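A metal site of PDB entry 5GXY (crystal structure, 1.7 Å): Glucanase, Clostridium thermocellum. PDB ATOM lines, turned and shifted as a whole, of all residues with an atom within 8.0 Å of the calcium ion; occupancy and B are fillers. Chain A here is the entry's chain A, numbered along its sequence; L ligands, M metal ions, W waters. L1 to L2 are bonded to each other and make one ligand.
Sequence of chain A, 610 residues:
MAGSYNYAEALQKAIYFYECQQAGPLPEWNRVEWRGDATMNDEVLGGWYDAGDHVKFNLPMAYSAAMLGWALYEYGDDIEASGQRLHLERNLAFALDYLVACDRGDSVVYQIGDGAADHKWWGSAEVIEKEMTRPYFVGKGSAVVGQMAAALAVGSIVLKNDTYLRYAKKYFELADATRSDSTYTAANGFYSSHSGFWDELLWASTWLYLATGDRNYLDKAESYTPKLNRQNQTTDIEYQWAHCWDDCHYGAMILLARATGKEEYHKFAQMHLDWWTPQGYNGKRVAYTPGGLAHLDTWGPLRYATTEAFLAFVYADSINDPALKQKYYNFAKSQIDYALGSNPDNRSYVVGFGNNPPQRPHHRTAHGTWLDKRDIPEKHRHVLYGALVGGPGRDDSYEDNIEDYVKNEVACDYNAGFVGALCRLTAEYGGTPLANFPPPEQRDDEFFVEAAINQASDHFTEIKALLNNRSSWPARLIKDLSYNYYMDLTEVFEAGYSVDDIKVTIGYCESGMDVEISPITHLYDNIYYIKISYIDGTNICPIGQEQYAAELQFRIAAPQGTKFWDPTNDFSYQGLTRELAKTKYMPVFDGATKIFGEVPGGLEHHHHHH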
ATOM      1  N   LEU A  59      -6.665 -12.302 -24.507  1.00  0.00           N
ATOM      2  CA  LEU A  59      -6.527 -10.977 -23.921  1.00  0.00           C
ATOM      3  C   LEU A  59      -5.949 -11.011 -22.487  1.00  0.00           C
ATOM      4  O   LEU A  59      -4.893 -10.438 -22.239  1.00  0.00           O
ATOM      5  CB  LEU A  59      -7.809 -10.125 -24.054  1.00  0.00           C
ATOM      6  CG  LEU A  59      -7.741  -8.686 -23.517  1.00  0.00           C
ATOM      7  CD1 LEU A  59      -6.631  -7.873 -24.188  1.00  0.00           C
ATOM      8  CD2 LEU A  59      -9.085  -7.968 -23.734  1.00  0.00           C
ATOM      9  N   SER A 142      -7.874  -5.179 -32.312  1.00  0.00           N
ATOM     10  CA  SER A 142      -6.763  -4.319 -31.917  1.00  0.00           C
ATOM     11  C   SER A 142      -6.434  -4.499 -30.433  1.00  0.00           C
ATOM     12  O   SER A 142      -5.258  -4.524 -30.083  1.00  0.00           O
ATOM     13  CB  SER A 142      -7.044  -2.855 -32.269  1.00  0.00           C
ATOM     14  OG  SER A 142      -7.162  -2.695 -33.688  1.00  0.00           O
ATOM     15  N   ALA A 143      -7.442  -4.634 -29.576  1.00  0.00           N
ATOM     16  CA  ALA A 143      -7.125  -4.860 -28.151  1.00  0.00           C
ATOM     17  C   ALA A 143      -6.394  -6.177 -27.880  1.00  0.00           C
ATOM     18  O   ALA A 143      -5.322  -6.186 -27.267  1.00  0.00           O
ATOM     19  CB  ALA A 143      -8.365  -4.717 -27.254  1.00  0.00           C
ATOM     20  N   VAL A 144      -6.931  -7.277 -28.387  1.00  0.00           N
ATOM     21  CA  VAL A 144      -6.303  -8.577 -28.125  1.00  0.00           C
ATOM     22  C   VAL A 144      -4.961  -8.700 -28.861  1.00  0.00           C
ATOM     23  O   VAL A 144      -3.983  -9.139 -28.275  1.00  0.00           O
ATOM     24  CB  VAL A 144      -7.253  -9.778 -28.368  1.00  0.00           C
ATOM     25  CG1 VAL A 144      -7.607  -9.944 -29.845  1.00  0.00           C
ATOM     26  CG2 VAL A 144      -6.667 -11.077 -27.793  1.00  0.00           C
ATOM     27  N   GLN A 147      -2.383  -6.341 -27.126  1.00  0.00           N
ATOM     28  CA  GLN A 147      -1.892  -6.907 -25.870  1.00  0.00           C
ATOM     29  C   GLN A 147      -0.887  -8.029 -26.150  1.00  0.00           C
ATOM     30  O   GLN A 147       0.133  -8.147 -25.466  1.00  0.00           O
ATOM     31  CB  GLN A 147      -3.040  -7.440 -24.992  1.00  0.00           C
ATOM     32  CG  GLN A 147      -2.579  -7.878 -23.591  1.00  0.00           C
ATOM     33  CD  GLN A 147      -1.979  -6.733 -22.780  1.00  0.00           C
ATOM     34  OE1 GLN A 147      -0.810  -6.802 -22.388  1.00  0.00           O
ATOM     35  NE2 GLN A 147      -2.754  -5.674 -22.543  1.00  0.00           N
ATOM     36  N   ASP A 181     -12.068  -3.321 -32.731  1.00  0.00           N
ATOM     37  CA  ASP A 181     -12.330  -4.559 -32.006  1.00  0.00           C
ATOM     38  C   ASP A 181     -13.488  -5.373 -32.590  1.00  0.00           C
ATOM     39  O   ASP A 181     -14.005  -6.273 -31.929  1.00  0.00           O
ATOM     40  CB  ASP A 181     -12.645  -4.252 -30.537  1.00  0.00           C
ATOM     41  CG  ASP A 181     -11.418  -3.893 -29.732  1.00  0.00           C
ATOM     42  OD1 ASP A 181     -10.322  -4.423 -30.050  1.00  0.00           O
ATOM     43  OD2 ASP A 181     -11.542  -3.086 -28.784  1.00  0.00           O
ATOM     44  N   SER A 192     -14.984  -9.158 -22.622  1.00  0.00           N
ATOM     45  CA  SER A 192     -15.353  -8.137 -23.609  1.00  0.00           C
ATOM     46  C   SER A 192     -14.358  -6.984 -23.578  1.00  0.00           C
ATOM     47  O   SER A 192     -13.801  -6.668 -22.518  1.00  0.00           O
ATOM     48  CB  SER A 192     -16.743  -7.574 -23.305  1.00  0.00           C
ATOM     49  OG  SER A 192     -17.737  -8.545 -23.563  1.00  0.00           O
ATOM     50  N   SER A 193     -14.136  -6.346 -24.718  1.00  0.00           N
ATOM     51  CA  SER A 193     -13.327  -5.139 -24.727  1.00  0.00           C
ATOM     52  C   SER A 193     -14.203  -3.976 -24.260  1.00  0.00           C
ATOM     53  O   SER A 193     -15.089  -3.497 -24.982  1.00  0.00           O
ATOM     54  CB  SER A 193     -12.723  -4.874 -26.120  1.00  0.00           C
ATOM     55  OG  SER A 193     -12.007  -3.645 -26.109  1.00  0.00           O
ATOM     56  N   HIS A 194     -13.967  -3.548 -23.021  1.00  0.00           N
ATOM     57  CA  HIS A 194     -14.787  -2.513 -22.389  1.00  0.00           C
ATOM     58  C   HIS A 194     -14.267  -1.107 -22.701  1.00  0.00           C
ATOM     59  O   HIS A 194     -15.055  -0.201 -22.986  1.00  0.00           O
ATOM     60  CB  HIS A 194     -14.818  -2.716 -20.872  1.00  0.00           C
ATOM     61  CG  HIS A 194     -15.445  -4.007 -20.447  1.00  0.00           C
ATOM     62  ND1 HIS A 194     -16.806  -4.146 -20.289  1.00  0.00           N
ATOM     63  CD2 HIS A 194     -14.898  -5.210 -20.160  1.00  0.00           C
ATOM     64  CE1 HIS A 194     -17.073  -5.388 -19.915  1.00  0.00           C
ATOM     65  NE2 HIS A 194     -15.930  -6.051 -19.824  1.00  0.00           N
ATOM     66  N   SER A 195     -12.960  -0.934 -22.645  1.00  0.00           N
ATOM     67  CA  SER A 195     -12.351   0.398 -22.741  1.00  0.00           C
ATOM     68  C   SER A 195     -12.013   0.729 -24.187  1.00  0.00           C
ATOM     69  O   SER A 195     -11.605   1.845 -24.485  1.00  0.00           O
ATOM     70  CB  SER A 195     -11.062   0.444 -21.908  1.00  0.00           C
ATOM     71  OG  SER A 195     -10.227  -0.682 -22.197  1.00  0.00           O
ATOM     72  N   GLY A 196     -12.186  -0.238 -25.093  1.00  0.00           N
ATOM     73  CA  GLY A 196     -11.693  -0.081 -26.463  1.00  0.00           C
ATOM     74  C   GLY A 196     -10.215  -0.406 -26.581  1.00  0.00           C
ATOM     75  O   GLY A 196      -9.628  -0.985 -25.661  1.00  0.00           O
ATOM     76  N   PHE A 197      -9.603  -0.036 -27.710  1.00  0.00           N
ATOM     77  CA  PHE A 197      -8.267  -0.545 -28.046  1.00  0.00           C
ATOM     78  C   PHE A 197      -7.152   0.496 -27.978  1.00  0.00           C
ATOM     79  O   PHE A 197      -5.980   0.141 -28.145  1.00  0.00           O
ATOM     80  CB  PHE A 197      -8.262  -1.187 -29.441  1.00  0.00           C
ATOM     81  CG  PHE A 197      -8.650  -0.228 -30.534  1.00  0.00           C
ATOM     82  CD1 PHE A 197      -7.757   0.737 -30.961  1.00  0.00           C
ATOM     83  CD2 PHE A 197      -9.935  -0.246 -31.048  1.00  0.00           C
ATOM     84  CE1 PHE A 197      -8.107   1.675 -31.934  1.00  0.00           C
ATOM     85  CE2 PHE A 197     -10.306   0.698 -32.016  1.00  0.00           C
ATOM     86  CZ  PHE A 197      -9.403   1.658 -32.435  1.00  0.00           C
ATOM     87  N   TRP A 198      -7.455   1.765 -27.751  1.00  0.00           N
ATOM     88  CA  TRP A 198      -6.370   2.745 -27.776  1.00  0.00           C
ATOM     89  C   TRP A 198      -5.356   2.513 -26.653  1.00  0.00           C
ATOM     90  O   TRP A 198      -4.165   2.753 -26.842  1.00  0.00           O
ATOM     91  CB  TRP A 198      -6.894   4.177 -27.758  1.00  0.00           C
ATOM     92  CG  TRP A 198      -7.733   4.501 -28.955  1.00  0.00           C
ATOM     93  CD1 TRP A 198      -9.094   4.628 -28.987  1.00  0.00           C
ATOM     94  CD2 TRP A 198      -7.280   4.738 -30.289  1.00  0.00           C
ATOM     95  NE1 TRP A 198      -9.515   4.925 -30.257  1.00  0.00           N
ATOM     96  CE2 TRP A 198      -8.423   5.008 -31.080  1.00  0.00           C
ATOM     97  CE3 TRP A 198      -6.018   4.755 -30.906  1.00  0.00           C
ATOM     98  CZ2 TRP A 198      -8.333   5.275 -32.453  1.00  0.00           C
ATOM     99  CZ3 TRP A 198      -5.940   5.029 -32.273  1.00  0.00           C
ATOM    100  CH2 TRP A 198      -7.093   5.290 -33.021  1.00  0.00           C
ATOM    101  N   ASP A 199      -5.833   2.091 -25.481  1.00  0.00           N
ATOM    102  CA  ASP A 199      -4.911   1.789 -24.382  1.00  0.00           C
ATOM    103  C   ASP A 199      -3.934   0.664 -24.712  1.00  0.00           C
ATOM    104  O   ASP A 199      -2.758   0.728 -24.347  1.00  0.00           O
ATOM    105  CB  ASP A 199      -5.687   1.477 -23.092  1.00  0.00           C
ATOM    106  CG  ASP A 199      -6.765   0.425 -23.307  1.00  0.00           C
ATOM    107  OD1 ASP A 199      -7.823   0.764 -23.889  1.00  0.00           O
ATOM    108  OD2 ASP A 199      -6.566  -0.755 -22.929  1.00  0.00           O
ATOM    109  N   GLU A 200      -4.401  -0.364 -25.404  1.00  0.00           N
ATOM    110  CA  GLU A 200      -3.513  -1.452 -25.853  1.00  0.00           C
ATOM    111  C   GLU A 200      -2.469  -0.938 -26.842  1.00  0.00           C
ATOM    112  O   GLU A 200      -1.297  -1.312 -26.749  1.00  0.00           O
ATOM    113  CB  GLU A 200      -4.290  -2.626 -26.455  1.00  0.00           C
ATOM    114  CG  GLU A 200      -5.038  -3.484 -25.420  1.00  0.00           C
ATOM    115  CD  GLU A 200      -6.402  -2.920 -25.029  1.00  0.00           C
ATOM    116  OE1 GLU A 200      -6.756  -1.833 -25.545  1.00  0.00           O
ATOM    117  OE2 GLU A 200      -7.129  -3.518 -24.189  1.00  0.00           O
ATOM    118  N   LEU A 201      -2.864  -0.069 -27.765  1.00  0.00           N
ATOM    119  CA  LEU A 201      -1.871   0.432 -28.712  1.00  0.00           C
ATOM    120  C   LEU A 201      -0.832   1.268 -27.995  1.00  0.00           C
ATOM    121  O   LEU A 201       0.358   1.181 -28.301  1.00  0.00           O
ATOM    122  CB  LEU A 201      -2.504   1.252 -29.849  1.00  0.00           C
ATOM    123  CG  LEU A 201      -3.472   0.476 -30.735  1.00  0.00           C
ATOM    124  CD1 LEU A 201      -4.056   1.462 -31.765  1.00  0.00           C
ATOM    125  CD2 LEU A 201      -2.803  -0.735 -31.429  1.00  0.00           C
ATOM    126  N   LEU A 228      -7.472   8.287 -25.451  1.00  0.00           N
ATOM    127  CA  LEU A 228      -7.862   7.514 -24.279  1.00  0.00           C
ATOM    128  C   LEU A 228      -9.195   8.016 -23.749  1.00  0.00           C
ATOM    129  O   LEU A 228      -9.533   9.198 -23.934  1.00  0.00           O
ATOM    130  CB  LEU A 228      -6.825   7.642 -23.165  1.00  0.00           C
ATOM    131  CG  LEU A 228      -5.451   7.051 -23.501  1.00  0.00           C
ATOM    132  CD1 LEU A 228      -4.400   7.475 -22.480  1.00  0.00           C
ATOM    133  CD2 LEU A 228      -5.548   5.530 -23.613  1.00  0.00           C
ATOM    134  N   ASN A 229      -9.907   7.145 -23.060  1.00  0.00           N
ATOM    135  CA  ASN A 229     -11.153   7.539 -22.402  1.00  0.00           C
ATOM    136  C   ASN A 229     -10.918   8.620 -21.351  1.00  0.00           C
ATOM    137  O   ASN A 229      -9.862   8.658 -20.703  1.00  0.00           O
ATOM    138  CB  ASN A 229     -11.876   6.324 -21.792  1.00  0.00           C
ATOM    139  CG  ASN A 229     -12.131   5.225 -22.806  1.00  0.00           C
ATOM    140  OD1 ASN A 229     -11.896   4.037 -22.547  1.00  0.00           O
ATOM    141  ND2 ASN A 229     -12.595   5.611 -23.984  1.00  0.00           N
ATOM    142  N   CYS A 244      -5.329  -3.341 -15.644  1.00  0.00           N
ATOM    143  CA  CYS A 244      -5.943  -4.670 -15.671  1.00  0.00           C
ATOM    144  C   CYS A 244      -5.949  -5.204 -17.096  1.00  0.00           C
ATOM    145  O   CYS A 244      -5.592  -4.493 -18.039  1.00  0.00           O
ATOM    146  CB  CYS A 244      -7.378  -4.643 -15.126  1.00  0.00           C
ATOM    147  SG  CYS A 244      -8.481  -3.605 -16.136  1.00  0.00           S
ATOM    148  N   TRP A 245      -6.395  -6.454 -17.232  1.00  0.00           N
ATOM    149  CA  TRP A 245      -6.481  -7.134 -18.526  1.00  0.00           C
ATOM    150  C   TRP A 245      -7.163  -6.336 -19.641  1.00  0.00           C
ATOM    151  O   TRP A 245      -6.831  -6.538 -20.809  1.00  0.00           O
ATOM    152  CB  TRP A 245      -7.148  -8.502 -18.392  1.00  0.00           C
ATOM    153  CG  TRP A 245      -8.565  -8.415 -17.941  1.00  0.00           C
ATOM    154  CD1 TRP A 245      -9.040  -8.524 -16.650  1.00  0.00           C
ATOM    155  CD2 TRP A 245      -9.718  -8.217 -18.773  1.00  0.00           C
ATOM    156  NE1 TRP A 245     -10.414  -8.384 -16.634  1.00  0.00           N
ATOM    157  CE2 TRP A 245     -10.844  -8.185 -17.926  1.00  0.00           C
ATOM    158  CE3 TRP A 245      -9.902  -8.029 -20.157  1.00  0.00           C
ATOM    159  CZ2 TRP A 245     -12.152  -7.992 -18.408  1.00  0.00           C
ATOM    160  CZ3 TRP A 245     -11.191  -7.834 -20.638  1.00  0.00           C
ATOM    161  CH2 TRP A 245     -12.296  -7.810 -19.760  1.00  0.00           C
ATOM    162  N   ASP A 246      -8.122  -5.492 -19.282  1.00  0.00           N
ATOM    163  CA  ASP A 246      -8.870  -4.694 -20.258  1.00  0.00           C
ATOM    164  C   ASP A 246      -8.249  -3.367 -20.631  1.00  0.00           C
ATOM    165  O   ASP A 246      -8.589  -2.776 -21.675  1.00  0.00           O
ATOM    166  CB  ASP A 246     -10.288  -4.424 -19.734  1.00  0.00           C
ATOM    167  CG  ASP A 246     -11.135  -3.717 -20.773  1.00  0.00           C
ATOM    168  OD1 ASP A 246     -11.425  -4.382 -21.787  1.00  0.00           O
ATOM    169  OD2 ASP A 246     -11.479  -2.533 -20.558  1.00  0.00           O
ATOM    170  N   ASP A 247      -7.393  -2.854 -19.749  1.00  0.00           N
ATOM    171  CA  ASP A 247      -6.953  -1.467 -19.798  1.00  0.00           C
ATOM    172  C   ASP A 247      -5.625  -1.269 -19.078  1.00  0.00           C
ATOM    173  O   ASP A 247      -5.552  -1.205 -17.852  1.00  0.00           O
ATOM    174  CB  ASP A 247      -8.030  -0.577 -19.152  1.00  0.00           C
ATOM    175  CG  ASP A 247      -7.811   0.898 -19.427  1.00  0.00           C
ATOM    176  OD1 ASP A 247      -6.725   1.295 -19.932  1.00  0.00           O
ATOM    177  OD2 ASP A 247      -8.731   1.669 -19.099  1.00  0.00           O
ATOM    178  N   CYS A 248      -4.567  -1.157 -19.879  1.00  0.00           N
ATOM    179  CA  CYS A 248      -3.230  -0.968 -19.365  1.00  0.00           C
ATOM    180  C   CYS A 248      -2.708   0.458 -19.537  1.00  0.00           C
ATOM    181  O   CYS A 248      -1.495   0.645 -19.431  1.00  0.00           O
ATOM    182  CB  CYS A 248      -2.274  -1.936 -20.064  1.00  0.00           C
ATOM    183  SG  CYS A 248      -2.512  -3.675 -19.622  1.00  0.00           S
ATOM    184  N   HIS A 249      -3.566   1.440 -19.802  1.00  0.00           N
ATOM    185  CA  HIS A 249      -3.038   2.805 -19.957  1.00  0.00           C
ATOM    186  C   HIS A 249      -2.380   3.315 -18.685  1.00  0.00           C
ATOM    187  O   HIS A 249      -1.397   4.043 -18.742  1.00  0.00           O
ATOM    188  CB  HIS A 249      -4.007   3.827 -20.549  1.00  0.00           C
ATOM    189  CG  HIS A 249      -5.012   4.391 -19.586  1.00  0.00           C
ATOM    190  ND1 HIS A 249      -6.228   3.809 -19.363  1.00  0.00           N
ATOM    191  CD2 HIS A 249      -5.013   5.556 -18.876  1.00  0.00           C
ATOM    192  CE1 HIS A 249      -6.925   4.552 -18.516  1.00  0.00           C
ATOM    193  NE2 HIS A 249      -6.214   5.616 -18.217  1.00  0.00           N
HETATM  194  C1  LIG L   1     -16.097  -5.097 -15.571  1.00  0.00           C
HETATM  195  C2  LIG L   1     -15.778  -3.930 -16.511  1.00  0.00           C
HETATM  196  C3  LIG L   1     -14.280  -3.646 -16.468  1.00  0.00           C
HETATM  197  C4  LIG L   1     -13.462  -4.922 -16.692  1.00  0.00           C
HETATM  198  C5  LIG L   1     -11.971  -4.726 -16.514  1.00  0.00           C
HETATM  199  C6  LIG L   1     -15.241  -6.304 -15.933  1.00  0.00           C
HETATM  200  O1  LIG L   1     -15.462  -7.353 -14.983  1.00  0.00           O
HETATM  201  O2  LIG L   1     -17.477  -5.438 -15.636  1.00  0.00           O
HETATM  202  O3  LIG L   1     -16.473  -2.760 -16.071  1.00  0.00           O
HETATM  203  O4  LIG L   1     -13.915  -2.699 -17.473  1.00  0.00           O
HETATM  204  O5  LIG L   1     -13.879  -5.915 -15.769  1.00  0.00           O
HETATM  205  O6  LIG L   1     -11.666  -4.326 -15.174  1.00  0.00           O
HETATM  206  C1  LG2 L   2     -12.657  -0.760 -18.015  1.00  0.00           C
HETATM  207  C2  LG2 L   2     -12.311   0.652 -17.558  1.00  0.00           C
HETATM  208  C3  LG2 L   2     -13.547   1.379 -17.026  1.00  0.00           C
HETATM  209  C4  LG2 L   2     -14.274   0.516 -15.996  1.00  0.00           C
HETATM  210  C5  LG2 L   2     -15.524   1.170 -15.419  1.00  0.00           C
HETATM  211  C6  LG2 L   2     -13.422  -1.480 -16.915  1.00  0.00           C
HETATM  212  O1  LG2 L   2     -11.419  -1.409 -18.314  1.00  0.00           O
HETATM  213  O2  LG2 L   2     -11.748   1.381 -18.656  1.00  0.00           O
HETATM  214  O3  LG2 L   2     -13.138   2.612 -16.417  1.00  0.00           O
HETATM  215  O4  LG2 L   2     -14.601  -0.730 -16.605  1.00  0.00           O
HETATM  216  O5  LG2 L   2     -16.498   1.274 -16.463  1.00  0.00           O
HETATM  217 CA    CA M   1      -8.534  -1.720 -23.745  1.00  0.00          CA
HETATM  218  O   HOH W   1     -10.237  -3.327 -23.986  1.00  0.00           O
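Water W1 bridges the side-chain carboxylate (OD1) of Asp 246 and the side-chain hydroxyl (OG) of Ser 193.
The backbone carbonyl oxygen (O) of Ser 195 lies close to the side-chain amide oxygen (OD1) of Asn 229, 2.9 Å away. The side-chain carboxylate (OD1) of Asp 246 is in hydrogen-bond range of the backbone NH (N) of His 194 (2.9 Å). The side-chain sulfur (SG) of Cys 244 sits close to the backbone NH (N) of Asp 246, at 3.7 Å.
The side-chain carboxylate of Asp 247 lies within hydrogen-bond range of an oxygen (O2) of LG2 L2 (3.1 Å). The side-chain sulfur (SG) of Cys 244 sits at hydrogen-bond distance from an oxygen (O6) of LIG L1 (3.4 Å). An oxygen (O1) of LG2 L2 is in hydrogen-bond range of the side-chain carboxylate (OD2) of Asp 246 (2.5 Å).
Of the 24 residues printed, 5 come within 4 Å of the calcium ion.
The calcium ion is bound by OE2 of Glu 200 (2.3 Å), O of Asp 246 (2.3 Å), O of Gly 196 (2.3 Å), OD2 of Asp 199 (2.3 Å), water W1 (2.4 Å), OG of Ser 195 (2.5 Å), OE1 of Glu 200 (2.5 Å) and OD1 of Asp 199 (2.6 Å).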
